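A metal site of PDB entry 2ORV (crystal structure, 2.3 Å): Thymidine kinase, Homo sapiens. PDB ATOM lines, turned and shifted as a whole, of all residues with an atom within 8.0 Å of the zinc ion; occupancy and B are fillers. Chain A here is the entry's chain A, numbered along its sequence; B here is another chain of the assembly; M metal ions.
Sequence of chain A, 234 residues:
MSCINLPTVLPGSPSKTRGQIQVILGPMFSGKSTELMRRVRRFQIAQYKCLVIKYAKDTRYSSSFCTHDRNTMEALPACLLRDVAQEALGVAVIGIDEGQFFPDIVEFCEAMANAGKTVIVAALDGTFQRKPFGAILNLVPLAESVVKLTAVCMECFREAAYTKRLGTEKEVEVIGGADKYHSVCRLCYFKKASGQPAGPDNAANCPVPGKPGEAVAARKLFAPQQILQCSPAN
NZ of Lys 164 lies within hydrogen-bond range of O of Cys 188, 3.2 Å away. The side-chain sulfur of Cys 185 sits close to the backbone NH of Leu 187 (3.5 Å). The backbone NH (N) of Arg 158 sits close to the side-chain sulfur (SG) of Cys 156, at 3.5 Å. The backbone carbonyl oxygen (O) of Arg 158 lies within hydrogen-bond range of the backbone NH (N) of Cys 153 (2.8 Å). The side-chain sulfur (SG) of Cys 153 sits close to the backbone NH (N) of Glu 155, 3.4 Å away.
Four residues have an atom within 4 Å of the zinc ion: Cys 153, Cys 156, Cys 185 and Cys 188. The nearest printed residue that does not touch the zinc ion is Glu 155 (4.6 Å).
The side-chain sulfur (SG) of Cys 156 binds the zinc ion (2.0 Å). The side-chain sulfur (SG) of Cys 188 is bound to the zinc ion (2.3 Å). The zinc ion is bound by SG of Cys 153, 2.5 Å away. The zinc ion is bound by SG of Cys 185. The zinc ion has four donor atoms within binding distance.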
ATOM      1  N   VAL A 152     -23.952  -3.554  -3.415  1.00  0.00           N
ATOM      2  CA  VAL A 152     -23.294  -2.806  -4.520  1.00  0.00           C
ATOM      3  C   VAL A 152     -22.509  -3.779  -5.382  1.00  0.00           C
ATOM      4  O   VAL A 152     -21.916  -4.726  -4.865  1.00  0.00           O
ATOM      5  CB  VAL A 152     -22.453  -1.573  -4.087  1.00  0.00           C
ATOM      6  CG1 VAL A 152     -22.687  -1.223  -2.657  1.00  0.00           C
ATOM      7  CG2 VAL A 152     -20.995  -1.732  -4.408  1.00  0.00           C
ATOM      8  N   CYS A 153     -22.557  -3.591  -6.695  1.00  0.00           N
ATOM      9  CA  CYS A 153     -21.906  -4.520  -7.590  1.00  0.00           C
ATOM     10  C   CYS A 153     -20.411  -4.542  -7.343  1.00  0.00           C
ATOM     11  O   CYS A 153     -19.763  -3.501  -7.302  1.00  0.00           O
ATOM     12  CB  CYS A 153     -22.199  -4.219  -9.066  1.00  0.00           C
ATOM     13  SG  CYS A 153     -21.561  -5.528 -10.128  1.00  0.00           S
ATOM     14  N   MET A 154     -19.868  -5.736  -7.153  1.00  0.00           N
ATOM     15  CA  MET A 154     -18.453  -5.896  -6.868  1.00  0.00           C
ATOM     16  C   MET A 154     -17.614  -5.821  -8.167  1.00  0.00           C
ATOM     17  O   MET A 154     -16.408  -5.835  -8.103  1.00  0.00           O
ATOM     18  CB  MET A 154     -18.200  -7.209  -6.116  1.00  0.00           C
ATOM     19  CG  MET A 154     -18.443  -7.118  -4.620  1.00  0.00           C
ATOM     20  SD  MET A 154     -18.512  -8.730  -3.769  1.00  0.00           S
ATOM     21  CE  MET A 154     -18.825  -8.159  -2.095  1.00  0.00           C
ATOM     22  N   GLU A 155     -18.248  -5.699  -9.332  1.00  0.00           N
ATOM     23  CA  GLU A 155     -17.509  -5.680 -10.584  1.00  0.00           C
ATOM     24  C   GLU A 155     -17.640  -4.393 -11.394  1.00  0.00           C
ATOM     25  O   GLU A 155     -16.709  -4.032 -12.115  1.00  0.00           O
ATOM     26  CB  GLU A 155     -17.845  -6.897 -11.442  1.00  0.00           C
ATOM     27  CG  GLU A 155     -17.173  -8.153 -10.966  1.00  0.00           C
ATOM     28  CD  GLU A 155     -17.901  -9.431 -11.358  1.00  0.00           C
ATOM     29  OE1 GLU A 155     -18.390  -9.545 -12.517  1.00  0.00           O
ATOM     30  OE2 GLU A 155     -17.953 -10.374 -10.515  1.00  0.00           O
ATOM     31  N   CYS A 156     -18.755  -3.676 -11.282  1.00  0.00           N
ATOM     32  CA  CYS A 156     -18.901  -2.385 -11.994  1.00  0.00           C
ATOM     33  C   CYS A 156     -19.276  -1.232 -11.063  1.00  0.00           C
ATOM     34  O   CYS A 156     -19.194  -0.060 -11.436  1.00  0.00           O
ATOM     35  CB  CYS A 156     -19.948  -2.498 -13.104  1.00  0.00           C
ATOM     36  SG  CYS A 156     -21.659  -2.648 -12.484  1.00  0.00           S
ATOM     37  N   PHE A 157     -19.694  -1.579  -9.839  1.00  0.00           N
ATOM     38  CA  PHE A 157     -20.076  -0.586  -8.821  1.00  0.00           C
ATOM     39  C   PHE A 157     -21.434   0.149  -9.053  1.00  0.00           C
ATOM     40  O   PHE A 157     -21.644   1.260  -8.554  1.00  0.00           O
ATOM     41  CB  PHE A 157     -18.925   0.418  -8.571  1.00  0.00           C
ATOM     42  CG  PHE A 157     -17.537  -0.215  -8.635  1.00  0.00           C
ATOM     43  CD1 PHE A 157     -16.623   0.177  -9.641  1.00  0.00           C
ATOM     44  CD2 PHE A 157     -17.162  -1.210  -7.724  1.00  0.00           C
ATOM     45  CE1 PHE A 157     -15.376  -0.414  -9.730  1.00  0.00           C
ATOM     46  CE2 PHE A 157     -15.908  -1.813  -7.809  1.00  0.00           C
ATOM     47  CZ  PHE A 157     -15.015  -1.408  -8.817  1.00  0.00           C
ATOM     48  N   ARG A 158     -22.368  -0.483  -9.773  1.00  0.00           N
ATOM     49  CA  ARG A 158     -23.760  -0.033  -9.762  1.00  0.00           C
ATOM     50  C   ARG A 158     -24.444  -0.729  -8.574  1.00  0.00           C
ATOM     51  O   ARG A 158     -23.775  -1.350  -7.761  1.00  0.00           O
ATOM     52  CB  ARG A 158     -24.442  -0.373 -11.087  1.00  0.00           C
ATOM     53  CG  ARG A 158     -23.729   0.195 -12.312  1.00  0.00           C
ATOM     54  CD  ARG A 158     -23.639   1.736 -12.293  1.00  0.00           C
ATOM     55  NE  ARG A 158     -22.782   2.277 -13.364  1.00  0.00           N
ATOM     56  CZ  ARG A 158     -21.593   2.845 -13.175  1.00  0.00           C
ATOM     57  NH1 ARG A 158     -21.058   2.936 -11.952  1.00  0.00           N
ATOM     58  NH2 ARG A 158     -20.912   3.306 -14.231  1.00  0.00           N
ATOM     59  N   GLU A 159     -25.754  -0.604  -8.440  1.00  0.00           N
ATOM     60  CA  GLU A 159     -26.444  -1.353  -7.393  1.00  0.00           C
ATOM     61  C   GLU A 159     -26.495  -2.832  -7.831  1.00  0.00           C
ATOM     62  O   GLU A 159     -26.576  -3.141  -9.035  1.00  0.00           O
ATOM     63  CB  GLU A 159     -27.840  -0.789  -7.157  1.00  0.00           C
ATOM     64  CG  GLU A 159     -27.822   0.555  -6.418  1.00  0.00           C
ATOM     65  CD  GLU A 159     -29.208   1.009  -5.905  1.00  0.00           C
ATOM     66  OE1 GLU A 159     -30.226   0.853  -6.653  1.00  0.00           O
ATOM     67  OE2 GLU A 159     -29.268   1.530  -4.736  1.00  0.00           O
ATOM     68  N   ALA A 160     -26.414  -3.742  -6.859  1.00  0.00           N
ATOM     69  CA  ALA A 160     -26.471  -5.153  -7.167  1.00  0.00           C
ATOM     70  C   ALA A 160     -27.741  -5.842  -6.642  1.00  0.00           C
ATOM     71  O   ALA A 160     -28.117  -5.695  -5.477  1.00  0.00           O
ATOM     72  CB  ALA A 160     -25.260  -5.852  -6.637  1.00  0.00           C
ATOM     73  N   LYS A 164     -23.554 -13.921  -7.839  1.00  0.00           N
ATOM     74  CA  LYS A 164     -22.801 -14.816  -8.743  1.00  0.00           C
ATOM     75  C   LYS A 164     -21.780 -15.697  -7.985  1.00  0.00           C
ATOM     76  O   LYS A 164     -21.028 -15.190  -7.167  1.00  0.00           O
ATOM     77  CB  LYS A 164     -22.041 -13.951  -9.746  1.00  0.00           C
ATOM     78  CG  LYS A 164     -21.082 -14.693 -10.638  1.00  0.00           C
ATOM     79  CD  LYS A 164     -20.774 -13.892 -11.917  1.00  0.00           C
ATOM     80  CE  LYS A 164     -19.734 -12.825 -11.703  1.00  0.00           C
ATOM     81  NZ  LYS A 164     -19.502 -12.089 -12.983  1.00  0.00           N
ATOM     82  N   SER A 183     -21.504 -10.034  -5.182  1.00  0.00           N
ATOM     83  CA  SER A 183     -22.792  -9.367  -5.349  1.00  0.00           C
ATOM     84  C   SER A 183     -22.731  -8.606  -6.658  1.00  0.00           C
ATOM     85  O   SER A 183     -21.762  -7.891  -6.947  1.00  0.00           O
ATOM     86  CB  SER A 183     -23.154  -8.442  -4.174  1.00  0.00           C
ATOM     87  OG  SER A 183     -22.233  -7.375  -4.029  1.00  0.00           O
ATOM     88  N   VAL A 184     -23.805  -8.740  -7.426  1.00  0.00           N
ATOM     89  CA  VAL A 184     -23.726  -8.380  -8.836  1.00  0.00           C
ATOM     90  C   VAL A 184     -25.047  -7.813  -9.450  1.00  0.00           C
ATOM     91  O   VAL A 184     -26.159  -8.301  -9.140  1.00  0.00           O
ATOM     92  CB  VAL A 184     -23.124  -9.624  -9.562  1.00  0.00           C
ATOM     93  CG1 VAL A 184     -24.143 -10.373 -10.355  1.00  0.00           C
ATOM     94  CG2 VAL A 184     -21.921  -9.215 -10.326  1.00  0.00           C
ATOM     95  N   CYS A 185     -24.915  -6.775 -10.285  1.00  0.00           N
ATOM     96  CA  CYS A 185     -26.014  -6.325 -11.157  1.00  0.00           C
ATOM     97  C   CYS A 185     -26.288  -7.293 -12.321  1.00  0.00           C
ATOM     98  O   CYS A 185     -25.525  -8.210 -12.562  1.00  0.00           O
ATOM     99  CB  CYS A 185     -25.723  -4.950 -11.725  1.00  0.00           C
ATOM    100  SG  CYS A 185     -24.463  -5.016 -13.048  1.00  0.00           S
ATOM    101  N   ARG A 186     -27.386  -7.053 -13.040  1.00  0.00           N
ATOM    102  CA  ARG A 186     -27.815  -7.813 -14.225  1.00  0.00           C
ATOM    103  C   ARG A 186     -26.715  -7.898 -15.274  1.00  0.00           C
ATOM    104  O   ARG A 186     -26.396  -8.964 -15.787  1.00  0.00           O
ATOM    105  CB  ARG A 186     -29.054  -7.128 -14.839  1.00  0.00           C
ATOM    106  CG  ARG A 186     -29.631  -7.812 -16.091  1.00  0.00           C
ATOM    107  CD  ARG A 186     -30.966  -7.205 -16.546  1.00  0.00           C
ATOM    108  NE  ARG A 186     -32.055  -7.356 -15.588  1.00  0.00           N
ATOM    109  CZ  ARG A 186     -32.859  -8.425 -15.474  1.00  0.00           C
ATOM    110  NH1 ARG A 186     -32.723  -9.502 -16.255  1.00  0.00           N
ATOM    111  NH2 ARG A 186     -33.824  -8.409 -14.562  1.00  0.00           N
ATOM    112  N   LEU A 187     -26.133  -6.745 -15.603  1.00  0.00           N
ATOM    113  CA  LEU A 187     -25.038  -6.699 -16.562  1.00  0.00           C
ATOM    114  C   LEU A 187     -23.868  -7.600 -16.192  1.00  0.00           C
ATOM    115  O   LEU A 187     -23.497  -8.489 -16.981  1.00  0.00           O
ATOM    116  CB  LEU A 187     -24.569  -5.275 -16.778  1.00  0.00           C
ATOM    117  CG  LEU A 187     -24.904  -4.774 -18.173  1.00  0.00           C
ATOM    118  CD1 LEU A 187     -25.439  -3.337 -18.117  1.00  0.00           C
ATOM    119  CD2 LEU A 187     -23.639  -4.889 -19.061  1.00  0.00           C
ATOM    120  N   CYS A 188     -23.307  -7.407 -15.006  1.00  0.00           N
ATOM    121  CA  CYS A 188     -22.146  -8.197 -14.581  1.00  0.00           C
ATOM    122  C   CYS A 188     -22.497  -9.652 -14.372  1.00  0.00           C
ATOM    123  O   CYS A 188     -21.699 -10.511 -14.679  1.00  0.00           O
ATOM    124  CB  CYS A 188     -21.499  -7.611 -13.338  1.00  0.00           C
ATOM    125  SG  CYS A 188     -20.806  -5.995 -13.613  1.00  0.00           S
ATOM    126  N   TYR A 189     -23.688  -9.944 -13.877  1.00  0.00           N
ATOM    127  CA  TYR A 189     -24.102 -11.333 -13.727  1.00  0.00           C
ATOM    128  C   TYR A 189     -23.843 -12.154 -14.977  1.00  0.00           C
ATOM    129  O   TYR A 189     -23.453 -13.307 -14.878  1.00  0.00           O
ATOM    130  CB  TYR A 189     -25.592 -11.429 -13.375  1.00  0.00           C
ATOM    131  CG  TYR A 189     -26.053 -12.829 -13.063  1.00  0.00           C
ATOM    132  CD1 TYR A 189     -25.920 -13.362 -11.780  1.00  0.00           C
ATOM    133  CD2 TYR A 189     -26.640 -13.620 -14.044  1.00  0.00           C
ATOM    134  CE1 TYR A 189     -26.336 -14.649 -11.475  1.00  0.00           C
ATOM    135  CE2 TYR A 189     -27.079 -14.913 -13.747  1.00  0.00           C
ATOM    136  CZ  TYR A 189     -26.924 -15.427 -12.466  1.00  0.00           C
ATOM    137  OH  TYR A 189     -27.348 -16.707 -12.181  1.00  0.00           O
ATOM    138  N   LYS A 191     -21.813 -11.312 -17.711  1.00  0.00           N
ATOM    139  CA  LYS A 191     -20.478 -11.128 -18.354  1.00  0.00           C
ATOM    140  C   LYS A 191     -19.686 -12.441 -18.534  1.00  0.00           C
ATOM    141  O   LYS A 191     -19.225 -13.048 -17.551  1.00  0.00           O
ATOM    142  CB  LYS A 191     -19.615 -10.114 -17.558  1.00  0.00           C
ATOM    143  CG  LYS A 191     -19.928  -8.639 -17.826  1.00  0.00           C
ATOM    144  CD  LYS A 191     -19.363  -8.154 -19.149  1.00  0.00           C
ATOM    145  CE  LYS A 191     -17.841  -7.858 -19.077  1.00  0.00           C
ATOM    146  NZ  LYS A 191     -17.474  -6.424 -18.740  1.00  0.00           N
ATOM    147  N   ARG B  18     -28.861  -0.529 -20.035  1.00  0.00           N
ATOM    148  CA  ARG B  18     -29.160  -1.462 -18.882  1.00  0.00           C
ATOM    149  C   ARG B  18     -30.673  -1.516 -18.487  1.00  0.00           C
ATOM    150  O   ARG B  18     -31.281  -0.508 -18.073  1.00  0.00           O
ATOM    151  CB  ARG B  18     -28.196  -1.223 -17.673  1.00  0.00           C
ATOM    152  CG  ARG B  18     -27.514   0.188 -17.586  1.00  0.00           C
ATOM    153  CD  ARG B  18     -26.872   0.471 -16.158  1.00  0.00           C
ATOM    154  NE  ARG B  18     -25.396   0.267 -16.072  1.00  0.00           N
ATOM    155  CZ  ARG B  18     -24.761  -0.554 -15.204  1.00  0.00           C
ATOM    156  NH1 ARG B  18     -25.432  -1.281 -14.314  1.00  0.00           N
ATOM    157  NH2 ARG B  18     -23.412  -0.637 -15.241  1.00  0.00           N
HETATM  158 ZN    ZN M   1     -22.119  -4.607 -12.334  1.00  0.00          ZN
